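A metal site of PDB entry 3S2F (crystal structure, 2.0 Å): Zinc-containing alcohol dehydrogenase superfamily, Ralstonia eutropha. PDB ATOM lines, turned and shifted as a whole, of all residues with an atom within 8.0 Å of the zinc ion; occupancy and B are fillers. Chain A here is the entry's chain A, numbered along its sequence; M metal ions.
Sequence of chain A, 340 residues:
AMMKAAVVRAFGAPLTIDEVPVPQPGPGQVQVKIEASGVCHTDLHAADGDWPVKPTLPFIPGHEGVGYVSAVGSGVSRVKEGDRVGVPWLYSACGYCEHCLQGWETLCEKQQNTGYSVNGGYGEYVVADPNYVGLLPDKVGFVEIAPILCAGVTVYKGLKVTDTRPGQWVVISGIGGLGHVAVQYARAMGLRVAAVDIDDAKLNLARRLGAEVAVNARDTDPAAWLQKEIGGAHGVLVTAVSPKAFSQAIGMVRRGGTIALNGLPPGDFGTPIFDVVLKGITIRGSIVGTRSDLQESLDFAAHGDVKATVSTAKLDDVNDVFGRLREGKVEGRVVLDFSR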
ATOM      1  N   SER A  92      -9.405   0.012  20.119  1.00  0.00           N
ATOM      2  CA  SER A  92      -8.345   0.847  20.675  1.00  0.00           C
ATOM      3  C   SER A  92      -7.480   0.048  21.640  1.00  0.00           C
ATOM      4  O   SER A  92      -7.889  -0.995  22.150  1.00  0.00           O
ATOM      5  CB  SER A  92      -8.960   2.056  21.395  1.00  0.00           C
ATOM      6  OG  SER A  92      -9.661   1.651  22.558  1.00  0.00           O
ATOM      7  N   ALA A  93      -6.270   0.541  21.868  1.00  0.00           N
ATOM      8  CA  ALA A  93      -5.379  -0.023  22.878  1.00  0.00           C
ATOM      9  C   ALA A  93      -4.818   1.123  23.709  1.00  0.00           C
ATOM     10  O   ALA A  93      -4.952   2.286  23.325  1.00  0.00           O
ATOM     11  CB  ALA A  93      -4.254  -0.815  22.211  1.00  0.00           C
ATOM     12  N   CYS A  94      -4.196   0.813  24.840  1.00  0.00           N
ATOM     13  CA  CYS A  94      -3.738   1.863  25.741  1.00  0.00           C
ATOM     14  C   CYS A  94      -2.545   2.627  25.169  1.00  0.00           C
ATOM     15  O   CYS A  94      -2.337   3.793  25.476  1.00  0.00           O
ATOM     16  CB  CYS A  94      -3.400   1.286  27.122  1.00  0.00           C
ATOM     17  SG  CYS A  94      -1.736   0.615  27.293  1.00  0.00           S
ATOM     18  N   GLY A  95      -1.770   1.954  24.306  1.00  0.00           N
ATOM     19  CA  GLY A  95      -0.652   2.587  23.617  1.00  0.00           C
ATOM     20  C   GLY A  95       0.602   2.758  24.448  1.00  0.00           C
ATOM     21  O   GLY A  95       1.638   3.199  23.943  1.00  0.00           O
ATOM     22  N   TYR A  96       0.537   2.381  25.726  1.00  0.00           N
ATOM     23  CA  TYR A  96       1.629   2.645  26.661  1.00  0.00           C
ATOM     24  C   TYR A  96       2.220   1.391  27.297  1.00  0.00           C
ATOM     25  O   TYR A  96       3.357   1.412  27.778  1.00  0.00           O
ATOM     26  CB  TYR A  96       1.179   3.617  27.747  1.00  0.00           C
ATOM     27  CG  TYR A  96       0.674   4.936  27.221  1.00  0.00           C
ATOM     28  CD1 TYR A  96      -0.448   5.546  27.764  1.00  0.00           C
ATOM     29  CD2 TYR A  96       1.319   5.574  26.172  1.00  0.00           C
ATOM     30  CE1 TYR A  96      -0.915   6.746  27.279  1.00  0.00           C
ATOM     31  CE2 TYR A  96       0.854   6.781  25.675  1.00  0.00           C
ATOM     32  CZ  TYR A  96      -0.258   7.367  26.238  1.00  0.00           C
ATOM     33  OH  TYR A  96      -0.734   8.563  25.758  1.00  0.00           O
ATOM     34  N   CYS A  97       1.456   0.300  27.315  1.00  0.00           N
ATOM     35  CA  CYS A  97       1.909  -0.916  27.975  1.00  0.00           C
ATOM     36  C   CYS A  97       3.054  -1.581  27.222  1.00  0.00           C
ATOM     37  O   CYS A  97       3.347  -1.233  26.079  1.00  0.00           O
ATOM     38  CB  CYS A  97       0.758  -1.907  28.161  1.00  0.00           C
ATOM     39  SG  CYS A  97       0.305  -2.794  26.650  1.00  0.00           S
ATOM     40  N   GLU A  98       3.681  -2.554  27.866  1.00  0.00           N
ATOM     41  CA  GLU A  98       4.761  -3.328  27.261  1.00  0.00           C
ATOM     42  C   GLU A  98       4.380  -3.890  25.896  1.00  0.00           C
ATOM     43  O   GLU A  98       5.195  -3.900  24.964  1.00  0.00           O
ATOM     44  CB  GLU A  98       5.173  -4.448  28.213  1.00  0.00           C
ATOM     45  CG  GLU A  98       5.568  -5.744  27.539  1.00  0.00           C
ATOM     46  CD  GLU A  98       6.041  -6.787  28.543  1.00  0.00           C
ATOM     47  OE1 GLU A  98       5.186  -7.541  29.068  1.00  0.00           O
ATOM     48  OE2 GLU A  98       7.257  -6.841  28.812  1.00  0.00           O
ATOM     49  N   HIS A  99       3.136  -4.340  25.766  1.00  0.00           N
ATOM     50  CA  HIS A  99       2.646  -4.895  24.512  1.00  0.00           C
ATOM     51  C   HIS A  99       2.487  -3.816  23.438  1.00  0.00           C
ATOM     52  O   HIS A  99       2.980  -3.970  22.317  1.00  0.00           O
ATOM     53  CB  HIS A  99       1.331  -5.620  24.736  1.00  0.00           C
ATOM     54  CG  HIS A  99       1.425  -6.769  25.693  1.00  0.00           C
ATOM     55  ND1 HIS A  99       2.401  -7.737  25.590  1.00  0.00           N
ATOM     56  CD2 HIS A  99       0.665  -7.113  26.756  1.00  0.00           C
ATOM     57  CE1 HIS A  99       2.243  -8.629  26.552  1.00  0.00           C
ATOM     58  NE2 HIS A  99       1.186  -8.273  27.276  1.00  0.00           N
ATOM     59  N   CYS A 100       1.811  -2.734  23.775  1.00  0.00           N
ATOM     60  CA  CYS A 100       1.562  -1.653  22.821  1.00  0.00           C
ATOM     61  C   CYS A 100       2.866  -1.041  22.309  1.00  0.00           C
ATOM     62  O   CYS A 100       2.993  -0.758  21.109  1.00  0.00           O
ATOM     63  CB  CYS A 100       0.675  -0.575  23.447  1.00  0.00           C
ATOM     64  SG  CYS A 100      -1.091  -0.969  23.414  1.00  0.00           S
ATOM     65  N   LEU A 101       3.817  -0.852  23.202  1.00  0.00           N
ATOM     66  CA  LEU A 101       5.111  -0.275  22.836  1.00  0.00           C
ATOM     67  C   LEU A 101       5.910  -1.196  21.919  1.00  0.00           C
ATOM     68  O   LEU A 101       6.734  -0.738  21.130  1.00  0.00           O
ATOM     69  CB  LEU A 101       5.921   0.072  24.086  1.00  0.00           C
ATOM     70  CG  LEU A 101       5.406   1.189  24.996  1.00  0.00           C
ATOM     71  CD1 LEU A 101       6.350   1.401  26.168  1.00  0.00           C
ATOM     72  CD2 LEU A 101       5.234   2.481  24.219  1.00  0.00           C
ATOM     73  N   TRP A 104       2.669  -4.929  19.568  1.00  0.00           N
ATOM     74  CA  TRP A 104       1.746  -6.041  19.720  1.00  0.00           C
ATOM     75  C   TRP A 104       0.470  -5.592  20.411  1.00  0.00           C
ATOM     76  O   TRP A 104       0.043  -6.167  21.415  1.00  0.00           O
ATOM     77  CB  TRP A 104       2.397  -7.182  20.518  1.00  0.00           C
ATOM     78  CG  TRP A 104       3.264  -8.075  19.674  1.00  0.00           C
ATOM     79  CD1 TRP A 104       4.602  -7.957  19.456  1.00  0.00           C
ATOM     80  CD2 TRP A 104       2.843  -9.234  18.948  1.00  0.00           C
ATOM     81  NE1 TRP A 104       5.037  -8.967  18.633  1.00  0.00           N
ATOM     82  CE2 TRP A 104       3.984  -9.760  18.310  1.00  0.00           C
ATOM     83  CE3 TRP A 104       1.609  -9.883  18.777  1.00  0.00           C
ATOM     84  CZ2 TRP A 104       3.921 -10.902  17.510  1.00  0.00           C
ATOM     85  CZ3 TRP A 104       1.553 -11.006  17.983  1.00  0.00           C
ATOM     86  CH2 TRP A 104       2.707 -11.506  17.363  1.00  0.00           C
ATOM     87  N   GLU A 105      -0.154  -4.549  19.863  1.00  0.00           N
ATOM     88  CA  GLU A 105      -1.338  -3.953  20.479  1.00  0.00           C
ATOM     89  C   GLU A 105      -2.504  -4.932  20.628  1.00  0.00           C
ATOM     90  O   GLU A 105      -3.437  -4.693  21.394  1.00  0.00           O
ATOM     91  CB  GLU A 105      -1.800  -2.709  19.700  1.00  0.00           C
ATOM     92  CG  GLU A 105      -2.101  -2.944  18.220  1.00  0.00           C
ATOM     93  CD  GLU A 105      -0.905  -2.665  17.327  1.00  0.00           C
ATOM     94  OE1 GLU A 105       0.234  -2.954  17.736  1.00  0.00           O
ATOM     95  OE2 GLU A 105      -1.115  -2.142  16.209  1.00  0.00           O
ATOM     96  N   THR A 106      -2.464  -6.026  19.870  1.00  0.00           N
ATOM     97  CA  THR A 106      -3.509  -7.048  19.964  1.00  0.00           C
ATOM     98  C   THR A 106      -3.519  -7.736  21.326  1.00  0.00           C
ATOM     99  O   THR A 106      -4.501  -8.374  21.697  1.00  0.00           O
ATOM    100  CB  THR A 106      -3.355  -8.114  18.855  1.00  0.00           C
ATOM    101  OG1 THR A 106      -1.986  -8.548  18.798  1.00  0.00           O
ATOM    102  CG2 THR A 106      -3.750  -7.544  17.518  1.00  0.00           C
ATOM    103  N   LEU A 107      -2.416  -7.605  22.059  1.00  0.00           N
ATOM    104  CA  LEU A 107      -2.270  -8.256  23.355  1.00  0.00           C
ATOM    105  C   LEU A 107      -2.516  -7.292  24.508  1.00  0.00           C
ATOM    106  O   LEU A 107      -2.377  -7.662  25.677  1.00  0.00           O
ATOM    107  CB  LEU A 107      -0.891  -8.890  23.485  1.00  0.00           C
ATOM    108  CG  LEU A 107      -0.519  -9.959  22.451  1.00  0.00           C
ATOM    109  CD1 LEU A 107       0.901 -10.465  22.680  1.00  0.00           C
ATOM    110  CD2 LEU A 107      -1.519 -11.117  22.482  1.00  0.00           C
ATOM    111  N   CYS A 108      -2.871  -6.048  24.184  1.00  0.00           N
ATOM    112  CA  CYS A 108      -3.134  -5.041  25.192  1.00  0.00           C
ATOM    113  C   CYS A 108      -4.295  -5.462  26.086  1.00  0.00           C
ATOM    114  O   CYS A 108      -5.387  -5.739  25.602  1.00  0.00           O
ATOM    115  CB  CYS A 108      -3.434  -3.682  24.561  1.00  0.00           C
ATOM    116  SG  CYS A 108      -3.950  -2.426  25.757  1.00  0.00           S
ATOM    117  N   GLU A 109      -4.037  -5.493  27.385  1.00  0.00           N
ATOM    118  CA  GLU A 109      -5.026  -5.954  28.354  1.00  0.00           C
ATOM    119  C   GLU A 109      -6.112  -4.904  28.600  1.00  0.00           C
ATOM    120  O   GLU A 109      -7.138  -5.196  29.227  1.00  0.00           O
ATOM    121  CB  GLU A 109      -4.338  -6.342  29.669  1.00  0.00           C
ATOM    122  CG  GLU A 109      -3.126  -7.239  29.453  1.00  0.00           C
ATOM    123  CD  GLU A 109      -2.813  -8.112  30.664  1.00  0.00           C
ATOM    124  OE1 GLU A 109      -2.420  -9.279  30.457  1.00  0.00           O
ATOM    125  OE2 GLU A 109      -2.953  -7.623  31.805  1.00  0.00           O
ATOM    126  N   LYS A 110      -5.884  -3.685  28.117  1.00  0.00           N
ATOM    127  CA  LYS A 110      -6.867  -2.613  28.260  1.00  0.00           C
ATOM    128  C   LYS A 110      -7.541  -2.283  26.927  1.00  0.00           C
ATOM    129  O   LYS A 110      -8.165  -1.228  26.788  1.00  0.00           O
ATOM    130  CB  LYS A 110      -6.214  -1.351  28.824  1.00  0.00           C
ATOM    131  CG  LYS A 110      -5.753  -1.471  30.260  1.00  0.00           C
ATOM    132  CD  LYS A 110      -5.314  -0.121  30.798  1.00  0.00           C
ATOM    133  CE  LYS A 110      -4.921  -0.215  32.262  1.00  0.00           C
ATOM    134  NZ  LYS A 110      -4.586   1.127  32.825  1.00  0.00           N
ATOM    135  N   GLN A 111      -7.414  -3.178  25.957  1.00  0.00           N
ATOM    136  CA  GLN A 111      -7.974  -2.958  24.636  1.00  0.00           C
ATOM    137  C   GLN A 111      -9.494  -2.933  24.690  1.00  0.00           C
ATOM    138  O   GLN A 111     -10.102  -3.560  25.557  1.00  0.00           O
ATOM    139  CB  GLN A 111      -7.498  -4.038  23.665  1.00  0.00           C
ATOM    140  CG  GLN A 111      -8.129  -5.403  23.882  1.00  0.00           C
ATOM    141  CD  GLN A 111      -7.579  -6.466  22.945  1.00  0.00           C
ATOM    142  OE1 GLN A 111      -8.216  -6.820  21.962  1.00  0.00           O
ATOM    143  NE2 GLN A 111      -6.402  -6.970  23.265  1.00  0.00           N
ATOM    144  N   TYR A 132      -6.709   3.498  15.021  1.00  0.00           N
ATOM    145  CA  TYR A 132      -6.866   2.048  14.976  1.00  0.00           C
ATOM    146  C   TYR A 132      -7.747   1.530  13.841  1.00  0.00           C
ATOM    147  O   TYR A 132      -7.884   0.320  13.665  1.00  0.00           O
ATOM    148  CB  TYR A 132      -7.373   1.525  16.322  1.00  0.00           C
ATOM    149  CG  TYR A 132      -6.355   1.684  17.415  1.00  0.00           C
ATOM    150  CD1 TYR A 132      -6.341   2.817  18.208  1.00  0.00           C
ATOM    151  CD2 TYR A 132      -5.399   0.703  17.649  1.00  0.00           C
ATOM    152  CE1 TYR A 132      -5.402   2.982  19.212  1.00  0.00           C
ATOM    153  CE2 TYR A 132      -4.458   0.851  18.642  1.00  0.00           C
ATOM    154  CZ  TYR A 132      -4.464   1.989  19.426  1.00  0.00           C
ATOM    155  OH  TYR A 132      -3.524   2.145  20.425  1.00  0.00           O
HETATM  156 ZN    ZN M   1      -1.637  -1.401  25.808  1.00  0.00          ZN
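Residues that only touch the zinc ion: Gly 95.
The zinc ion is bound by the side-chain sulfur (SG) of Cys 100, the side-chain sulfur (SG) of Cys 94, the side-chain sulfur (SG) of Cys 108 and the side-chain sulfur (SG) of Cys 97. The zinc ion has four donor atoms within binding distance.
SG of Cys 100 sits close to N of Gly 95. The backbone NH of Tyr 96 sits close to the side-chain sulfur of Cys 94 (3.3 Å). N of Lys 110 lies close to SG of Cys 108 (3.3 Å). The backbone carbonyl oxygen of Cys 108 sits at hydrogen-bond distance from the side-chain amide nitrogen of Gln 111, 2.8 Å away. SG of Cys 97 lies close to N of His 99 (3.3 Å).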
